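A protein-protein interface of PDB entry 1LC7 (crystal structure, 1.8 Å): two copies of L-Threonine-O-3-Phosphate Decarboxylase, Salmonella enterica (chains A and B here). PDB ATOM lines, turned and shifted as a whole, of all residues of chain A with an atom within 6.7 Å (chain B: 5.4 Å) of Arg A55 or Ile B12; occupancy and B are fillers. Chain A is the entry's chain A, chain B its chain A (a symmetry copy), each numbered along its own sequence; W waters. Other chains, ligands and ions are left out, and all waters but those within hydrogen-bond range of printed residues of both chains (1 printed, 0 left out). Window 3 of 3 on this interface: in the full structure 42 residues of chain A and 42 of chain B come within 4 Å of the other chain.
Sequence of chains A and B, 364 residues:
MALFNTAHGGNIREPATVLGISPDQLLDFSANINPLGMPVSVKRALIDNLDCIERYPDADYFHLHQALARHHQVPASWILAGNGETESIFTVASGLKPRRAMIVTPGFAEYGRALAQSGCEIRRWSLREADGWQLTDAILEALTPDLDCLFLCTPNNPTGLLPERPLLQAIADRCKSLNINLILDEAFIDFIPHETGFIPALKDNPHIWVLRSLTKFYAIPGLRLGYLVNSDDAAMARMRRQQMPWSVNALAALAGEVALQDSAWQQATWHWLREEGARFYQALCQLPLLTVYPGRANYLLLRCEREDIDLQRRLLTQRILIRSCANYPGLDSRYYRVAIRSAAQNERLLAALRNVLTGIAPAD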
ATOM      1  N   ASP A  51     -11.332  -3.236   3.890  1.00  0.00           N
ATOM      2  CA  ASP A  51     -11.795  -1.872   4.092  1.00  0.00           C
ATOM      3  C   ASP A  51     -13.312  -1.760   4.253  1.00  0.00           C
ATOM      4  O   ASP A  51     -13.804  -0.708   4.646  1.00  0.00           O
ATOM      5  CB  ASP A  51     -11.327  -0.971   2.929  1.00  0.00           C
ATOM      6  N   CYS A  52     -14.045  -2.828   3.953  1.00  0.00           N
ATOM      7  CA  CYS A  52     -15.489  -2.777   4.112  1.00  0.00           C
ATOM      8  C   CYS A  52     -15.887  -2.619   5.583  1.00  0.00           C
ATOM      9  O   CYS A  52     -17.031  -2.293   5.875  1.00  0.00           O
ATOM     10  CB  CYS A  52     -16.159  -4.022   3.502  1.00  0.00           C
ATOM     11  SG  CYS A  52     -16.047  -5.536   4.455  1.00  0.00           S
ATOM     12  N   ILE A  53     -14.956  -2.810   6.516  1.00  0.00           N
ATOM     13  CA  ILE A  53     -15.314  -2.667   7.922  1.00  0.00           C
ATOM     14  C   ILE A  53     -15.429  -1.201   8.362  1.00  0.00           C
ATOM     15  O   ILE A  53     -15.864  -0.891   9.493  1.00  0.00           O
ATOM     16  CB  ILE A  53     -14.323  -3.417   8.838  1.00  0.00           C
ATOM     17  CG1 ILE A  53     -12.920  -2.818   8.690  1.00  0.00           C
ATOM     18  CG2 ILE A  53     -14.339  -4.904   8.502  1.00  0.00           C
ATOM     19  CD1 ILE A  53     -11.934  -3.329   9.720  1.00  0.00           C
ATOM     20  N   GLU A  54     -15.042  -0.294   7.459  1.00  0.00           N
ATOM     21  CA  GLU A  54     -15.116   1.148   7.708  1.00  0.00           C
ATOM     22  C   GLU A  54     -16.559   1.644   7.588  1.00  0.00           C
ATOM     23  O   GLU A  54     -16.884   2.791   7.926  1.00  0.00           O
ATOM     24  CB  GLU A  54     -14.199   1.892   6.724  1.00  0.00           C
ATOM     25  CG  GLU A  54     -12.736   1.758   7.121  1.00  0.00           C
ATOM     26  CD  GLU A  54     -11.778   2.453   6.174  1.00  0.00           C
ATOM     27  OE1 GLU A  54     -10.581   2.518   6.502  1.00  0.00           O
ATOM     28  OE2 GLU A  54     -12.217   2.922   5.109  1.00  0.00           O
ATOM     29  N   ARG A  55     -17.438   0.779   7.098  1.00  0.00           N
ATOM     30  CA  ARG A  55     -18.839   1.156   7.007  1.00  0.00           C
ATOM     31  C   ARG A  55     -19.631   0.096   7.760  1.00  0.00           C
ATOM     32  O   ARG A  55     -19.125  -1.017   7.970  1.00  0.00           O
ATOM     33  CB  ARG A  55     -19.277   1.173   5.552  1.00  0.00           C
ATOM     34  CG  ARG A  55     -18.413   2.075   4.654  1.00  0.00           C
ATOM     35  CD  ARG A  55     -19.022   2.149   3.266  1.00  0.00           C
ATOM     36  NE  ARG A  55     -19.544   0.848   2.876  1.00  0.00           N
ATOM     37  CZ  ARG A  55     -18.808  -0.165   2.432  1.00  0.00           C
ATOM     38  NH1 ARG A  55     -17.491  -0.043   2.295  1.00  0.00           N
ATOM     39  NH2 ARG A  55     -19.401  -1.317   2.147  1.00  0.00           N
ATOM     40  N   TYR A  56     -20.849   0.446   8.167  1.00  0.00           N
ATOM     41  CA  TYR A  56     -21.746  -0.504   8.830  1.00  0.00           C
ATOM     42  C   TYR A  56     -22.125  -1.573   7.801  1.00  0.00           C
ATOM     43  O   TYR A  56     -22.072  -1.335   6.605  1.00  0.00           O
ATOM     44  CB  TYR A  56     -23.080   0.164   9.237  1.00  0.00           C
ATOM     45  CG  TYR A  56     -23.109   0.862  10.573  1.00  0.00           C
ATOM     46  CD1 TYR A  56     -22.775   2.203  10.698  1.00  0.00           C
ATOM     47  CD2 TYR A  56     -23.437   0.154  11.730  1.00  0.00           C
ATOM     48  CE1 TYR A  56     -22.760   2.832  11.963  1.00  0.00           C
ATOM     49  CE2 TYR A  56     -23.415   0.755  12.984  1.00  0.00           C
ATOM     50  CZ  TYR A  56     -23.075   2.092  13.093  1.00  0.00           C
ATOM     51  OH  TYR A  56     -23.014   2.629  14.362  1.00  0.00           O
ATOM     52  N   PRO A  57     -22.508  -2.766   8.262  1.00  0.00           N
ATOM     53  CA  PRO A  57     -22.912  -3.818   7.322  1.00  0.00           C
ATOM     54  C   PRO A  57     -24.275  -3.340   6.806  1.00  0.00           C
ATOM     55  O   PRO A  57     -24.845  -2.408   7.362  1.00  0.00           O
ATOM     56  CB  PRO A  57     -23.106  -5.042   8.220  1.00  0.00           C
ATOM     57  CG  PRO A  57     -22.318  -4.728   9.471  1.00  0.00           C
ATOM     58  CD  PRO A  57     -22.535  -3.253   9.647  1.00  0.00           C
ATOM     59  N   ALA A 250     -19.608  -7.321   8.881  1.00  0.00           N
ATOM     60  CA  ALA A 250     -19.373  -7.238   7.439  1.00  0.00           C
ATOM     61  C   ALA A 250     -18.488  -8.332   6.847  1.00  0.00           C
ATOM     62  O   ALA A 250     -18.753  -8.799   5.735  1.00  0.00           O
ATOM     63  CB  ALA A 250     -18.797  -5.863   7.098  1.00  0.00           C
ATOM     64  N   GLY B  10     -26.773   5.280   7.506  1.00  0.00           N
ATOM     65  CA  GLY B  10     -25.788   4.390   6.941  1.00  0.00           C
ATOM     66  C   GLY B  10     -26.354   3.391   5.928  1.00  0.00           C
ATOM     67  O   GLY B  10     -25.617   2.526   5.433  1.00  0.00           O
ATOM     68  N   ASN B  11     -27.631   3.527   5.582  1.00  0.00           N
ATOM     69  CA  ASN B  11     -28.282   2.591   4.655  1.00  0.00           C
ATOM     70  C   ASN B  11     -27.977   2.878   3.190  1.00  0.00           C
ATOM     71  O   ASN B  11     -28.890   3.136   2.400  1.00  0.00           O
ATOM     72  CB  ASN B  11     -29.808   2.589   4.907  1.00  0.00           C
ATOM     73  CG  ASN B  11     -30.466   3.965   4.708  1.00  0.00           C
ATOM     74  OD1 ASN B  11     -29.909   5.005   5.066  1.00  0.00           O
ATOM     75  ND2 ASN B  11     -31.682   3.958   4.167  1.00  0.00           N
ATOM     76  N   ILE B  12     -26.699   2.810   2.826  1.00  0.00           N
ATOM     77  CA  ILE B  12     -26.319   3.146   1.449  1.00  0.00           C
ATOM     78  C   ILE B  12     -26.815   2.174   0.419  1.00  0.00           C
ATOM     79  O   ILE B  12     -27.137   2.588  -0.692  1.00  0.00           O
ATOM     80  CB  ILE B  12     -24.797   3.298   1.291  1.00  0.00           C
ATOM     81  CG1 ILE B  12     -24.087   2.002   1.679  1.00  0.00           C
ATOM     82  CG2 ILE B  12     -24.330   4.445   2.149  1.00  0.00           C
ATOM     83  CD1 ILE B  12     -22.618   1.972   1.370  1.00  0.00           C
ATOM     84  N   ARG B  13     -26.873   0.890   0.765  1.00  0.00           N
ATOM     85  CA  ARG B  13     -27.360  -0.111  -0.197  1.00  0.00           C
ATOM     86  C   ARG B  13     -28.833   0.191  -0.469  1.00  0.00           C
ATOM     87  O   ARG B  13     -29.271   0.178  -1.630  1.00  0.00           O
ATOM     88  CB  ARG B  13     -27.170  -1.540   0.380  1.00  0.00           C
ATOM     89  CG  ARG B  13     -27.313  -2.714  -0.625  1.00  0.00           C
ATOM     90  CD  ARG B  13     -28.759  -3.143  -0.766  1.00  0.00           C
ATOM     91  NE  ARG B  13     -29.337  -3.344   0.548  1.00  0.00           N
ATOM     92  CZ  ARG B  13     -30.610  -3.121   0.859  1.00  0.00           C
ATOM     93  NH1 ARG B  13     -31.466  -2.699  -0.065  1.00  0.00           N
ATOM     94  NH2 ARG B  13     -31.005  -3.248   2.117  1.00  0.00           N
ATOM     95  N   GLU B  14     -29.605   0.497   0.576  1.00  0.00           N
ATOM     96  CA  GLU B  14     -31.038   0.787   0.380  1.00  0.00           C
ATOM     97  C   GLU B  14     -31.272   2.071  -0.416  1.00  0.00           C
ATOM     98  O   GLU B  14     -32.164   2.135  -1.278  1.00  0.00           O
ATOM     99  CB  GLU B  14     -31.778   0.915   1.722  1.00  0.00           C
ATOM    100  CG  GLU B  14     -33.277   1.122   1.512  1.00  0.00           C
ATOM    101  CD  GLU B  14     -34.062   1.315   2.793  1.00  0.00           C
ATOM    102  OE1 GLU B  14     -35.297   1.144   2.744  1.00  0.00           O
ATOM    103  OE2 GLU B  14     -33.463   1.641   3.835  1.00  0.00           O
ATOM    104  N   PRO B  15     -30.474   3.093  -0.114  1.00  0.00           N
ATOM    105  CA  PRO B  15     -30.576   4.381  -0.799  1.00  0.00           C
ATOM    106  C   PRO B  15     -30.208   4.259  -2.280  1.00  0.00           C
ATOM    107  O   PRO B  15     -30.912   4.770  -3.151  1.00  0.00           O
ATOM    108  CB  PRO B  15     -29.665   5.396  -0.127  1.00  0.00           C
ATOM    109  N   ALA B  16     -29.105   3.583  -2.553  1.00  0.00           N
ATOM    110  CA  ALA B  16     -28.658   3.380  -3.909  1.00  0.00           C
ATOM    111  C   ALA B  16     -29.734   2.609  -4.674  1.00  0.00           C
ATOM    112  O   ALA B  16     -30.019   2.922  -5.823  1.00  0.00           O
ATOM    113  CB  ALA B  16     -27.339   2.611  -3.901  1.00  0.00           C
ATOM    114  N   THR B  17     -30.346   1.609  -4.041  1.00  0.00           N
ATOM    115  CA  THR B  17     -31.400   0.838  -4.709  1.00  0.00           C
ATOM    116  C   THR B  17     -32.614   1.704  -5.066  1.00  0.00           C
ATOM    117  O   THR B  17     -33.278   1.479  -6.077  1.00  0.00           O
ATOM    118  CB  THR B  17     -31.845  -0.361  -3.841  1.00  0.00           C
ATOM    119  OG1 THR B  17     -30.747  -1.260  -3.690  1.00  0.00           O
ATOM    120  CG2 THR B  17     -32.980  -1.117  -4.507  1.00  0.00           C
ATOM    121  N   PRO B  23     -24.147   1.400  -4.655  1.00  0.00           N
ATOM    122  CA  PRO B  23     -23.873   2.095  -3.393  1.00  0.00           C
ATOM    123  C   PRO B  23     -22.575   2.884  -3.417  1.00  0.00           C
ATOM    124  O   PRO B  23     -22.449   3.905  -2.743  1.00  0.00           O
ATOM    125  CB  PRO B  23     -23.830   0.956  -2.364  1.00  0.00           C
ATOM    126  CG  PRO B  23     -24.723  -0.100  -2.976  1.00  0.00           C
ATOM    127  CD  PRO B  23     -24.293  -0.049  -4.428  1.00  0.00           C
ATOM    128  N   LEU B  26     -22.686   6.736  -3.953  1.00  0.00           N
ATOM    129  CA  LEU B  26     -23.223   7.711  -2.995  1.00  0.00           C
ATOM    130  C   LEU B  26     -22.171   8.200  -2.007  1.00  0.00           C
ATOM    131  O   LEU B  26     -21.258   7.445  -1.641  1.00  0.00           O
ATOM    132  CB  LEU B  26     -24.378   7.109  -2.207  1.00  0.00           C
ATOM    133  CG  LEU B  26     -25.636   6.784  -2.999  1.00  0.00           C
ATOM    134  CD1 LEU B  26     -26.632   6.051  -2.084  1.00  0.00           C
ATOM    135  CD2 LEU B  26     -26.257   8.077  -3.525  1.00  0.00           C
ATOM    136  N   ASP B  28     -21.949   9.277   1.652  1.00  0.00           N
ATOM    137  CA  ASP B  28     -22.768   9.093   2.847  1.00  0.00           C
ATOM    138  C   ASP B  28     -22.459   9.974   4.037  1.00  0.00           C
ATOM    139  O   ASP B  28     -21.390   9.876   4.636  1.00  0.00           O
ATOM    140  CB  ASP B  28     -22.700   7.619   3.266  1.00  0.00           C
ATOM    141  CG  ASP B  28     -23.785   7.239   4.274  1.00  0.00           C
ATOM    142  OD1 ASP B  28     -24.727   8.035   4.444  1.00  0.00           O
ATOM    143  OD2 ASP B  28     -23.695   6.138   4.855  1.00  0.00           O
ATOM    144  N   ILE B  33     -19.139   8.094  11.072  1.00  0.00           N
ATOM    145  CA  ILE B  33     -17.901   7.335  11.240  1.00  0.00           C
ATOM    146  C   ILE B  33     -16.694   8.259  11.042  1.00  0.00           C
ATOM    147  O   ILE B  33     -16.687   9.069  10.110  1.00  0.00           O
ATOM    148  CB  ILE B  33     -17.827   6.190  10.193  1.00  0.00           C
ATOM    149  CG1 ILE B  33     -19.132   5.366  10.191  1.00  0.00           C
ATOM    150  CG2 ILE B  33     -16.658   5.273  10.522  1.00  0.00           C
ATOM    151  CD1 ILE B  33     -19.448   4.754  11.533  1.00  0.00           C
ATOM    152  N   PRO B 221     -17.092   0.278  12.160  1.00  0.00           N
ATOM    153  CA  PRO B 221     -18.481  -0.112  12.372  1.00  0.00           C
ATOM    154  C   PRO B 221     -18.837  -1.466  11.798  1.00  0.00           C
ATOM    155  O   PRO B 221     -19.791  -2.102  12.253  1.00  0.00           O
ATOM    156  CB  PRO B 221     -19.259   1.022  11.718  1.00  0.00           C
ATOM    157  CG  PRO B 221     -18.359   1.470  10.635  1.00  0.00           C
ATOM    158  CD  PRO B 221     -17.008   1.489  11.326  1.00  0.00           C
ATOM    159  N   GLY B 222     -18.089  -1.894  10.779  1.00  0.00           N
ATOM    160  CA  GLY B 222     -18.374  -3.182  10.164  1.00  0.00           C
ATOM    161  C   GLY B 222     -17.931  -4.370  10.991  1.00  0.00           C
ATOM    162  O   GLY B 222     -18.375  -5.494  10.744  1.00  0.00           O
ATOM    163  N   LEU B 321     -26.283  11.180   0.576  1.00  0.00           N
ATOM    164  CA  LEU B 321     -27.250  10.638   1.527  1.00  0.00           C
ATOM    165  C   LEU B 321     -27.100  11.290   2.889  1.00  0.00           C
ATOM    166  O   LEU B 321     -26.010  11.291   3.460  1.00  0.00           O
ATOM    167  CB  LEU B 321     -27.027   9.121   1.672  1.00  0.00           C
ATOM    168  CG  LEU B 321     -27.901   8.395   2.713  1.00  0.00           C
ATOM    169  CD1 LEU B 321     -29.375   8.584   2.347  1.00  0.00           C
ATOM    170  CD2 LEU B 321     -27.531   6.878   2.745  1.00  0.00           C
HETATM  171  O   HOH W   1     -26.059  -0.322   6.176  1.00  0.00           O
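The backbone carbonyl oxygen (O) of Ile A53 lies close to the backbone nitrogen (N) of Pro B221 (3.2 Å).
O of Gly B222 is in hydrogen-bond range of N of Ala A250, 2.9 Å away.
The backbone carbonyl oxygen of Ile A53 is in hydrogen-bond range of the backbone NH of Gly B222 (2.8 Å).
The backbone carbonyl oxygen of Arg A55 is in hydrogen-bond range of the backbone NH of Gly B222, at 3.1 Å.
Glu A54 touches Ile B33.
Pro B221 touches Glu A54 (CG to O, 3.4 Å).
Ile B12 touches Arg A55 (CD1 to NE, 3.6 Å).
C of Arg A55 touches CG of Pro B221, at 3.4 Å.
Tyr A56 touches Ile B33.
N of Tyr A56 touches CG of Pro B221 (3.7 Å).
CD of Pro A57 touches O of Pro B221 (3.96 Å).
Of the printed residues of chain B, Ile A53 touches Pro B221 (3.2 Å) and Gly B222 (2.8 Å).
Printed residues of chain B within 4 Å of Glu A54: Ile B33 and Pro B221.
Arg A55 touches three residues of chain B.
Ile B12 touches just one residue of chain A: Arg A55.
Printed residues of chain A within 4 Å of Ile B33: Glu A54 and Tyr A56.
Of the printed residues of chain A, Pro B221 touches Ile A53, Glu A54, Arg A55, Tyr A56 and Pro A57.
Of the printed residues of chain A, Gly B222 touches Ile A53, Arg A55 and Ala A250.
Of the 8 printed residues of chain A, 6 touch a printed residue of chain B.
Hydrophobic or aromatic side chains of chain A that line the printed part of chain B: Tyr A56, Pro A57 and Ala A250.
Printed residues of chain B that touch a printed residue of chain A: Ile B12, Ile B33, Pro B221 and Gly B222.
Hydrophobic or aromatic side chains of chain B within 4 Å of the printed part of chain A: Ile B12, Ile B33 and Pro B221.
Among the printed residues, 11 pairs touch across the chains.
No position is printed for both chains.
Of the 11 pairs that touch across the chains among the printed residues, none has its exchanged pair printed and touching as well.
Water W1 bridges O of Pro A57 (2.7 Å) and O of Gly B10 (3.0 Å).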
